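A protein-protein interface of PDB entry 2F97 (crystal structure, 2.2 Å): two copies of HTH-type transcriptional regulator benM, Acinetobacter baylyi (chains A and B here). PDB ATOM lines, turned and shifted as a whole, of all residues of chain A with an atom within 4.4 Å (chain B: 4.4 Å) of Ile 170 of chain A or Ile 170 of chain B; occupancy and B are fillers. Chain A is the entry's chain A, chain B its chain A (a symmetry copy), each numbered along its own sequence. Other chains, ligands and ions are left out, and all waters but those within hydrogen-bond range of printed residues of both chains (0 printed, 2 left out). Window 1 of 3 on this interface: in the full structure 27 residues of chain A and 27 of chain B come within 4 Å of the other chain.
O of Ser 169 of chain A is in hydrogen-bond range of N of Gln 171 of chain B (2.9 Å).
The backbone NH (N) of Gln 171 of chain A is in hydrogen-bond range of the backbone carbonyl oxygen (O) of Ser 169 of chain B, 2.9 Å away.
The backbone carbonyl oxygen (O) of Ser 169 of chain B lies close to the backbone carbonyl oxygen (O) of Ser 169 of chain A, 3.3 Å away.
The backbone carbonyl oxygen (O) of Phe 22 of chain A sits at hydrogen-bond distance from the side-chain hydroxyl (OG) of Ser 169 of chain A, 2.9 Å away.
O of Gln 168 of chain A is in hydrogen-bond range of NE2 of Gln 171 of chain A (2.9 Å).
O of Ile 170 of chain A lies within hydrogen-bond range of OH of Tyr 177 of chain A, 2.7 Å away.
The side-chain hydroxyl (OG) of Ser 169 of chain B is in hydrogen-bond range of the backbone carbonyl oxygen (O) of Phe 22 of chain B (2.9 Å).
O of Gln 168 of chain B is in hydrogen-bond range of NE2 of Gln 171 of chain B (2.9 Å).
The side-chain hydroxyl (OH) of Tyr 177 of chain B lies within hydrogen-bond range of the backbone carbonyl oxygen (O) of Ile 170 of chain B.
Among the printed residues, merely in contact across the chains: Phe 22 of chain A with Leu 172 of chain B, Ser 169 of chain A with Ile 170 of chain B, Ser 169 of chain A with Leu 172 of chain B, Ile 170 of chain A with Ser 169 of chain B, Ile 170 of chain A with Ile 170 of chain B, Leu 172 of chain A with Phe 22 of chain B and Leu 172 of chain A with Ser 169 of chain B.
Of the printed residues of chain B, Phe 22 of chain A touches Leu 172 (3.9 Å).
Printed residues of chain B within 4 Å of Ser 169 of chain A: Ser 169 (3.3 Å), Ile 170 (3.5 Å), Gln 171 (2.9 Å) and Leu 172 (3.8 Å).
Of chain B, only Ser 169 and Ile 170 come within 4 Å of Ile 170 of chain A.
Of the printed residues of chain B, Leu 172 of chain A touches Phe 22 (3.9 Å) and Ser 169 (3.8 Å).
Printed residues of chain A within 4 Å of Phe 22 of chain B: Leu 172.
Gln 168 of chain B touches none of the printed residues of chain A.
Printed residues of chain A within 4 Å of Ser 169 of chain B: Ser 169 (3.3 Å), Ile 170 (3.5 Å), Gln 171 (2.9 Å) and Leu 172 (3.8 Å).
Ile 170 of chain B touches just these residues of chain A: Ser 169 (3.5 Å) and Ile 170 (3.9 Å).
Leu 175 of chain B touches none of the printed residues of chain A.
The nearest printed residue of chain B that does not touch Leu 172 of chain A is Ile 170 of chain B (6.3 Å).
Hydrophobic or aromatic side chains of chain A that line the printed part of chain B: Ile 170 and Leu 172.
Among the printed residues, 10 pairs touch across the chains.
Among the printed residues, no Asp or Glu carboxylate lies within 4 Å of a Lys or Arg side-chain nitrogen of the other chain.
Phe 22 of chain A touches Leu 172 of chain B, and with the chains exchanged Leu 172 of chain A touches Phe 22 of chain B.
Ser 169 of chain A touches Gln 171 of chain B, and with the chains exchanged Gln 171 of chain A touches Ser 169 of chain B.
Ser 169 of chain A touches Leu 172 of chain B, and with the chains exchanged Leu 172 of chain A touches Ser 169 of chain B.
Ile 170 of chain B touches its own counterpart, Ile 170 of chain A.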
ATOM      1  N   PHE A  22      -9.078  -1.975  -7.904  1.00  0.00           N
ATOM      2  CA  PHE A  22      -8.871  -1.310  -6.618  1.00  0.00           C
ATOM      3  C   PHE A  22      -8.923  -2.282  -5.439  1.00  0.00           C
ATOM      4  O   PHE A  22      -8.618  -1.907  -4.302  1.00  0.00           O
ATOM      5  CB  PHE A  22      -9.892  -0.182  -6.423  1.00  0.00           C
ATOM      6  CG  PHE A  22      -9.889   0.838  -7.529  1.00  0.00           C
ATOM      7  CD1 PHE A  22      -8.819   1.716  -7.682  1.00  0.00           C
ATOM      8  CD2 PHE A  22     -10.956   0.919  -8.417  1.00  0.00           C
ATOM      9  CE1 PHE A  22      -8.813   2.661  -8.708  1.00  0.00           C
ATOM     10  CE2 PHE A  22     -10.963   1.860  -9.447  1.00  0.00           C
ATOM     11  CZ  PHE A  22      -9.890   2.733  -9.592  1.00  0.00           C
ATOM     12  N   LEU A 151     -15.567  10.691  -8.523  1.00  0.00           N
ATOM     13  CA  LEU A 151     -14.952  11.068  -7.243  1.00  0.00           C
ATOM     14  C   LEU A 151     -14.397  12.498  -7.262  1.00  0.00           C
ATOM     15  O   LEU A 151     -14.591  13.255  -6.308  1.00  0.00           O
ATOM     16  CB  LEU A 151     -13.869  10.061  -6.838  1.00  0.00           C
ATOM     17  CG  LEU A 151     -14.335   8.615  -6.588  1.00  0.00           C
ATOM     18  CD1 LEU A 151     -13.150   7.706  -6.318  1.00  0.00           C
ATOM     19  CD2 LEU A 151     -15.340   8.537  -5.436  1.00  0.00           C
ATOM     20  N   THR A 167     -12.972   0.899  -3.589  1.00  0.00           N
ATOM     21  CA  THR A 167     -12.679   2.164  -4.281  1.00  0.00           C
ATOM     22  C   THR A 167     -12.080   3.213  -3.321  1.00  0.00           C
ATOM     23  O   THR A 167     -11.564   4.249  -3.757  1.00  0.00           O
ATOM     24  CB  THR A 167     -13.928   2.676  -5.060  1.00  0.00           C
ATOM     25  OG1 THR A 167     -14.180   1.803  -6.171  1.00  0.00           O
ATOM     26  CG2 THR A 167     -13.732   4.087  -5.593  1.00  0.00           C
ATOM     27  N   GLN A 168     -12.116   2.917  -2.020  1.00  0.00           N
ATOM     28  CA  GLN A 168     -11.423   3.721  -1.005  1.00  0.00           C
ATOM     29  C   GLN A 168      -9.897   3.680  -1.163  1.00  0.00           C
ATOM     30  O   GLN A 168      -9.169   4.355  -0.429  1.00  0.00           O
ATOM     31  CB  GLN A 168     -11.811   3.267   0.401  1.00  0.00           C
ATOM     32  CG  GLN A 168     -13.233   3.623   0.793  1.00  0.00           C
ATOM     33  CD  GLN A 168     -13.626   3.018   2.117  1.00  0.00           C
ATOM     34  OE1 GLN A 168     -13.842   1.811   2.224  1.00  0.00           O
ATOM     35  NE2 GLN A 168     -13.725   3.852   3.135  1.00  0.00           N
ATOM     36  N   SER A 169      -9.423   2.882  -2.118  1.00  0.00           N
ATOM     37  CA  SER A 169      -8.036   2.951  -2.578  1.00  0.00           C
ATOM     38  C   SER A 169      -7.710   4.343  -3.123  1.00  0.00           C
ATOM     39  O   SER A 169      -6.549   4.761  -3.122  1.00  0.00           O
ATOM     40  CB  SER A 169      -7.780   1.895  -3.651  1.00  0.00           C
ATOM     41  OG  SER A 169      -7.793   0.596  -3.084  1.00  0.00           O
ATOM     42  N   ILE A 170      -8.744   5.051  -3.583  1.00  0.00           N
ATOM     43  CA  ILE A 170      -8.618   6.438  -4.026  1.00  0.00           C
ATOM     44  C   ILE A 170      -9.016   7.379  -2.894  1.00  0.00           C
ATOM     45  O   ILE A 170     -10.176   7.399  -2.469  1.00  0.00           O
ATOM     46  CB  ILE A 170      -9.487   6.742  -5.279  1.00  0.00           C
ATOM     47  CG1 ILE A 170      -9.162   5.768  -6.419  1.00  0.00           C
ATOM     48  CG2 ILE A 170      -9.307   8.209  -5.717  1.00  0.00           C
ATOM     49  CD1 ILE A 170     -10.009   5.954  -7.682  1.00  0.00           C
ATOM     50  N   GLN A 171      -8.047   8.146  -2.404  1.00  0.00           N
ATOM     51  CA  GLN A 171      -8.303   9.125  -1.356  1.00  0.00           C
ATOM     52  C   GLN A 171      -7.997  10.516  -1.893  1.00  0.00           C
ATOM     53  O   GLN A 171      -6.911  10.755  -2.419  1.00  0.00           O
ATOM     54  CB  GLN A 171      -7.465   8.823  -0.105  1.00  0.00           C
ATOM     55  CG  GLN A 171      -7.844   7.526   0.618  1.00  0.00           C
ATOM     56  CD  GLN A 171      -9.190   7.602   1.334  1.00  0.00           C
ATOM     57  OE1 GLN A 171      -9.541   8.627   1.918  1.00  0.00           O
ATOM     58  NE2 GLN A 171      -9.942   6.506   1.297  1.00  0.00           N
ATOM     59  N   LEU A 172      -8.967  11.420  -1.776  1.00  0.00           N
ATOM     60  CA  LEU A 172      -8.817  12.794  -2.262  1.00  0.00           C
ATOM     61  C   LEU A 172      -9.150  13.777  -1.152  1.00  0.00           C
ATOM     62  O   LEU A 172      -9.981  13.482  -0.283  1.00  0.00           O
ATOM     63  CB  LEU A 172      -9.736  13.056  -3.465  1.00  0.00           C
ATOM     64  CG  LEU A 172      -9.759  12.097  -4.661  1.00  0.00           C
ATOM     65  CD1 LEU A 172     -10.883  12.480  -5.621  1.00  0.00           C
ATOM     66  CD2 LEU A 172      -8.419  12.068  -5.389  1.00  0.00           C
ATOM     67  N   LEU A 175     -12.708  14.493   0.321  1.00  0.00           N
ATOM     68  CA  LEU A 175     -13.565  13.395  -0.109  1.00  0.00           C
ATOM     69  C   LEU A 175     -13.699  12.417   1.047  1.00  0.00           C
ATOM     70  O   LEU A 175     -12.699  11.979   1.617  1.00  0.00           O
ATOM     71  CB  LEU A 175     -12.998  12.691  -1.351  1.00  0.00           C
ATOM     72  CG  LEU A 175     -13.746  11.456  -1.873  1.00  0.00           C
ATOM     73  CD1 LEU A 175     -15.071  11.853  -2.514  1.00  0.00           C
ATOM     74  CD2 LEU A 175     -12.893  10.652  -2.862  1.00  0.00           C
ATOM     75  N   TYR A 177     -15.920   8.880   2.621  1.00  0.00           N
ATOM     76  CA  TYR A 177     -16.741   7.713   2.301  1.00  0.00           C
ATOM     77  C   TYR A 177     -17.638   7.346   3.477  1.00  0.00           C
ATOM     78  O   TYR A 177     -17.168   7.180   4.605  1.00  0.00           O
ATOM     79  CB  TYR A 177     -15.871   6.523   1.897  1.00  0.00           C
ATOM     80  CG  TYR A 177     -15.070   6.721   0.627  1.00  0.00           C
ATOM     81  CD1 TYR A 177     -15.624   6.433  -0.622  1.00  0.00           C
ATOM     82  CD2 TYR A 177     -13.749   7.174   0.674  1.00  0.00           C
ATOM     83  CE1 TYR A 177     -14.888   6.600  -1.791  1.00  0.00           C
ATOM     84  CE2 TYR A 177     -13.002   7.343  -0.493  1.00  0.00           C
ATOM     85  CZ  TYR A 177     -13.580   7.054  -1.720  1.00  0.00           C
ATOM     86  OH  TYR A 177     -12.855   7.213  -2.878  1.00  0.00           O
ATOM     87  N   PHE B  22      -6.760  14.247  -9.231  1.00  0.00           N
ATOM     88  CA  PHE B  22      -6.067  13.653  -8.087  1.00  0.00           C
ATOM     89  C   PHE B  22      -5.279  14.681  -7.277  1.00  0.00           C
ATOM     90  O   PHE B  22      -4.763  14.370  -6.198  1.00  0.00           O
ATOM     91  CB  PHE B  22      -5.144  12.517  -8.547  1.00  0.00           C
ATOM     92  CG  PHE B  22      -5.847  11.443  -9.331  1.00  0.00           C
ATOM     93  CD1 PHE B  22      -6.742  10.577  -8.707  1.00  0.00           C
ATOM     94  CD2 PHE B  22      -5.613  11.296 -10.694  1.00  0.00           C
ATOM     95  CE1 PHE B  22      -7.397   9.582  -9.432  1.00  0.00           C
ATOM     96  CE2 PHE B  22      -6.261  10.304 -11.432  1.00  0.00           C
ATOM     97  CZ  PHE B  22      -7.153   9.445 -10.799  1.00  0.00           C
ATOM     98  N   LEU B 151      -1.999   1.447 -13.281  1.00  0.00           N
ATOM     99  CA  LEU B 151      -1.626   1.146 -11.891  1.00  0.00           C
ATOM    100  C   LEU B 151      -2.032  -0.272 -11.472  1.00  0.00           C
ATOM    101  O   LEU B 151      -1.250  -0.983 -10.837  1.00  0.00           O
ATOM    102  CB  LEU B 151      -2.203   2.193 -10.931  1.00  0.00           C
ATOM    103  CG  LEU B 151      -1.714   3.641 -11.117  1.00  0.00           C
ATOM    104  CD1 LEU B 151      -2.455   4.585 -10.189  1.00  0.00           C
ATOM    105  CD2 LEU B 151      -0.203   3.759 -10.903  1.00  0.00           C
ATOM    106  N   THR B 167      -0.942  11.523  -8.350  1.00  0.00           N
ATOM    107  CA  THR B 167      -1.590  10.231  -8.619  1.00  0.00           C
ATOM    108  C   THR B 167      -1.401   9.243  -7.449  1.00  0.00           C
ATOM    109  O   THR B 167      -2.057   8.196  -7.391  1.00  0.00           O
ATOM    110  CB  THR B 167      -1.139   9.656  -9.996  1.00  0.00           C
ATOM    111  OG1 THR B 167      -1.688  10.467 -11.046  1.00  0.00           O
ATOM    112  CG2 THR B 167      -1.609   8.224 -10.201  1.00  0.00           C
ATOM    113  N   GLN B 168      -0.532   9.604  -6.502  1.00  0.00           N
ATOM    114  CA  GLN B 168      -0.383   8.866  -5.241  1.00  0.00           C
ATOM    115  C   GLN B 168      -1.645   8.927  -4.370  1.00  0.00           C
ATOM    116  O   GLN B 168      -1.707   8.303  -3.306  1.00  0.00           O
ATOM    117  CB  GLN B 168       0.819   9.383  -4.452  1.00  0.00           C
ATOM    118  CG  GLN B 168       2.159   9.021  -5.062  1.00  0.00           C
ATOM    119  CD  GLN B 168       3.308   9.684  -4.345  1.00  0.00           C
ATOM    120  OE1 GLN B 168       3.519  10.891  -4.466  1.00  0.00           O
ATOM    121  NE2 GLN B 168       4.061   8.901  -3.597  1.00  0.00           N
ATOM    122  N   SER B 169      -2.641   9.684  -4.825  1.00  0.00           N
ATOM    123  CA  SER B 169      -3.992   9.618  -4.268  1.00  0.00           C
ATOM    124  C   SER B 169      -4.568   8.206  -4.398  1.00  0.00           C
ATOM    125  O   SER B 169      -5.441   7.811  -3.621  1.00  0.00           O
ATOM    126  CB  SER B 169      -4.904  10.623  -4.967  1.00  0.00           C
ATOM    127  OG  SER B 169      -4.550  11.948  -4.612  1.00  0.00           O
ATOM    128  N   ILE B 170      -4.069   7.457  -5.383  1.00  0.00           N
ATOM    129  CA  ILE B 170      -4.427   6.052  -5.566  1.00  0.00           C
ATOM    130  C   ILE B 170      -3.371   5.162  -4.921  1.00  0.00           C
ATOM    131  O   ILE B 170      -2.213   5.141  -5.352  1.00  0.00           O
ATOM    132  CB  ILE B 170      -4.577   5.668  -7.066  1.00  0.00           C
ATOM    133  CG1 ILE B 170      -5.584   6.590  -7.767  1.00  0.00           C
ATOM    134  CG2 ILE B 170      -4.972   4.185  -7.207  1.00  0.00           C
ATOM    135  CD1 ILE B 170      -5.759   6.324  -9.266  1.00  0.00           C
ATOM    136  N   GLN B 171      -3.772   4.440  -3.880  1.00  0.00           N
ATOM    137  CA  GLN B 171      -2.878   3.510  -3.203  1.00  0.00           C
ATOM    138  C   GLN B 171      -3.433   2.099  -3.340  1.00  0.00           C
ATOM    139  O   GLN B 171      -4.596   1.855  -3.020  1.00  0.00           O
ATOM    140  CB  GLN B 171      -2.705   3.890  -1.725  1.00  0.00           C
ATOM    141  CG  GLN B 171      -1.971   5.215  -1.490  1.00  0.00           C
ATOM    142  CD  GLN B 171      -0.483   5.150  -1.820  1.00  0.00           C
ATOM    143  OE1 GLN B 171       0.183   4.150  -1.553  1.00  0.00           O
ATOM    144  NE2 GLN B 171       0.044   6.228  -2.393  1.00  0.00           N
ATOM    145  N   LEU B 172      -2.604   1.184  -3.837  1.00  0.00           N
ATOM    146  CA  LEU B 172      -3.008  -0.209  -4.038  1.00  0.00           C
ATOM    147  C   LEU B 172      -2.015  -1.141  -3.364  1.00  0.00           C
ATOM    148  O   LEU B 172      -0.825  -0.818  -3.261  1.00  0.00           O
ATOM    149  CB  LEU B 172      -3.089  -0.549  -5.535  1.00  0.00           C
ATOM    150  CG  LEU B 172      -3.868   0.348  -6.504  1.00  0.00           C
ATOM    151  CD1 LEU B 172      -3.632  -0.104  -7.943  1.00  0.00           C
ATOM    152  CD2 LEU B 172      -5.359   0.364  -6.185  1.00  0.00           C
ATOM    153  N   LEU B 175       1.657  -1.848  -4.527  1.00  0.00           N
ATOM    154  CA  LEU B 175       2.008  -0.790  -5.466  1.00  0.00           C
ATOM    155  C   LEU B 175       2.843   0.243  -4.727  1.00  0.00           C
ATOM    156  O   LEU B 175       2.447   0.728  -3.667  1.00  0.00           O
ATOM    157  CB  LEU B 175       0.756  -0.139  -6.074  1.00  0.00           C
ATOM    158  CG  LEU B 175       0.961   1.054  -7.018  1.00  0.00           C
ATOM    159  CD1 LEU B 175       1.556   0.601  -8.346  1.00  0.00           C
ATOM    160  CD2 LEU B 175      -0.346   1.822  -7.253  1.00  0.00           C
ATOM    161  N   TYR B 177       5.487   3.813  -5.160  1.00  0.00           N
ATOM    162  CA  TYR B 177       5.880   4.947  -5.995  1.00  0.00           C
ATOM    163  C   TYR B 177       7.319   5.356  -5.707  1.00  0.00           C
ATOM    164  O   TYR B 177       7.694   5.588  -4.555  1.00  0.00           O
ATOM    165  CB  TYR B 177       4.935   6.131  -5.796  1.00  0.00           C
ATOM    166  CG  TYR B 177       3.504   5.884  -6.226  1.00  0.00           C
ATOM    167  CD1 TYR B 177       3.106   6.098  -7.548  1.00  0.00           C
ATOM    168  CD2 TYR B 177       2.540   5.458  -5.308  1.00  0.00           C
ATOM    169  CE1 TYR B 177       1.790   5.885  -7.946  1.00  0.00           C
ATOM    170  CE2 TYR B 177       1.217   5.245  -5.697  1.00  0.00           C
ATOM    171  CZ  TYR B 177       0.852   5.461  -7.018  1.00  0.00           C
ATOM    172  OH  TYR B 177      -0.450   5.256  -7.415  1.00  0.00           O
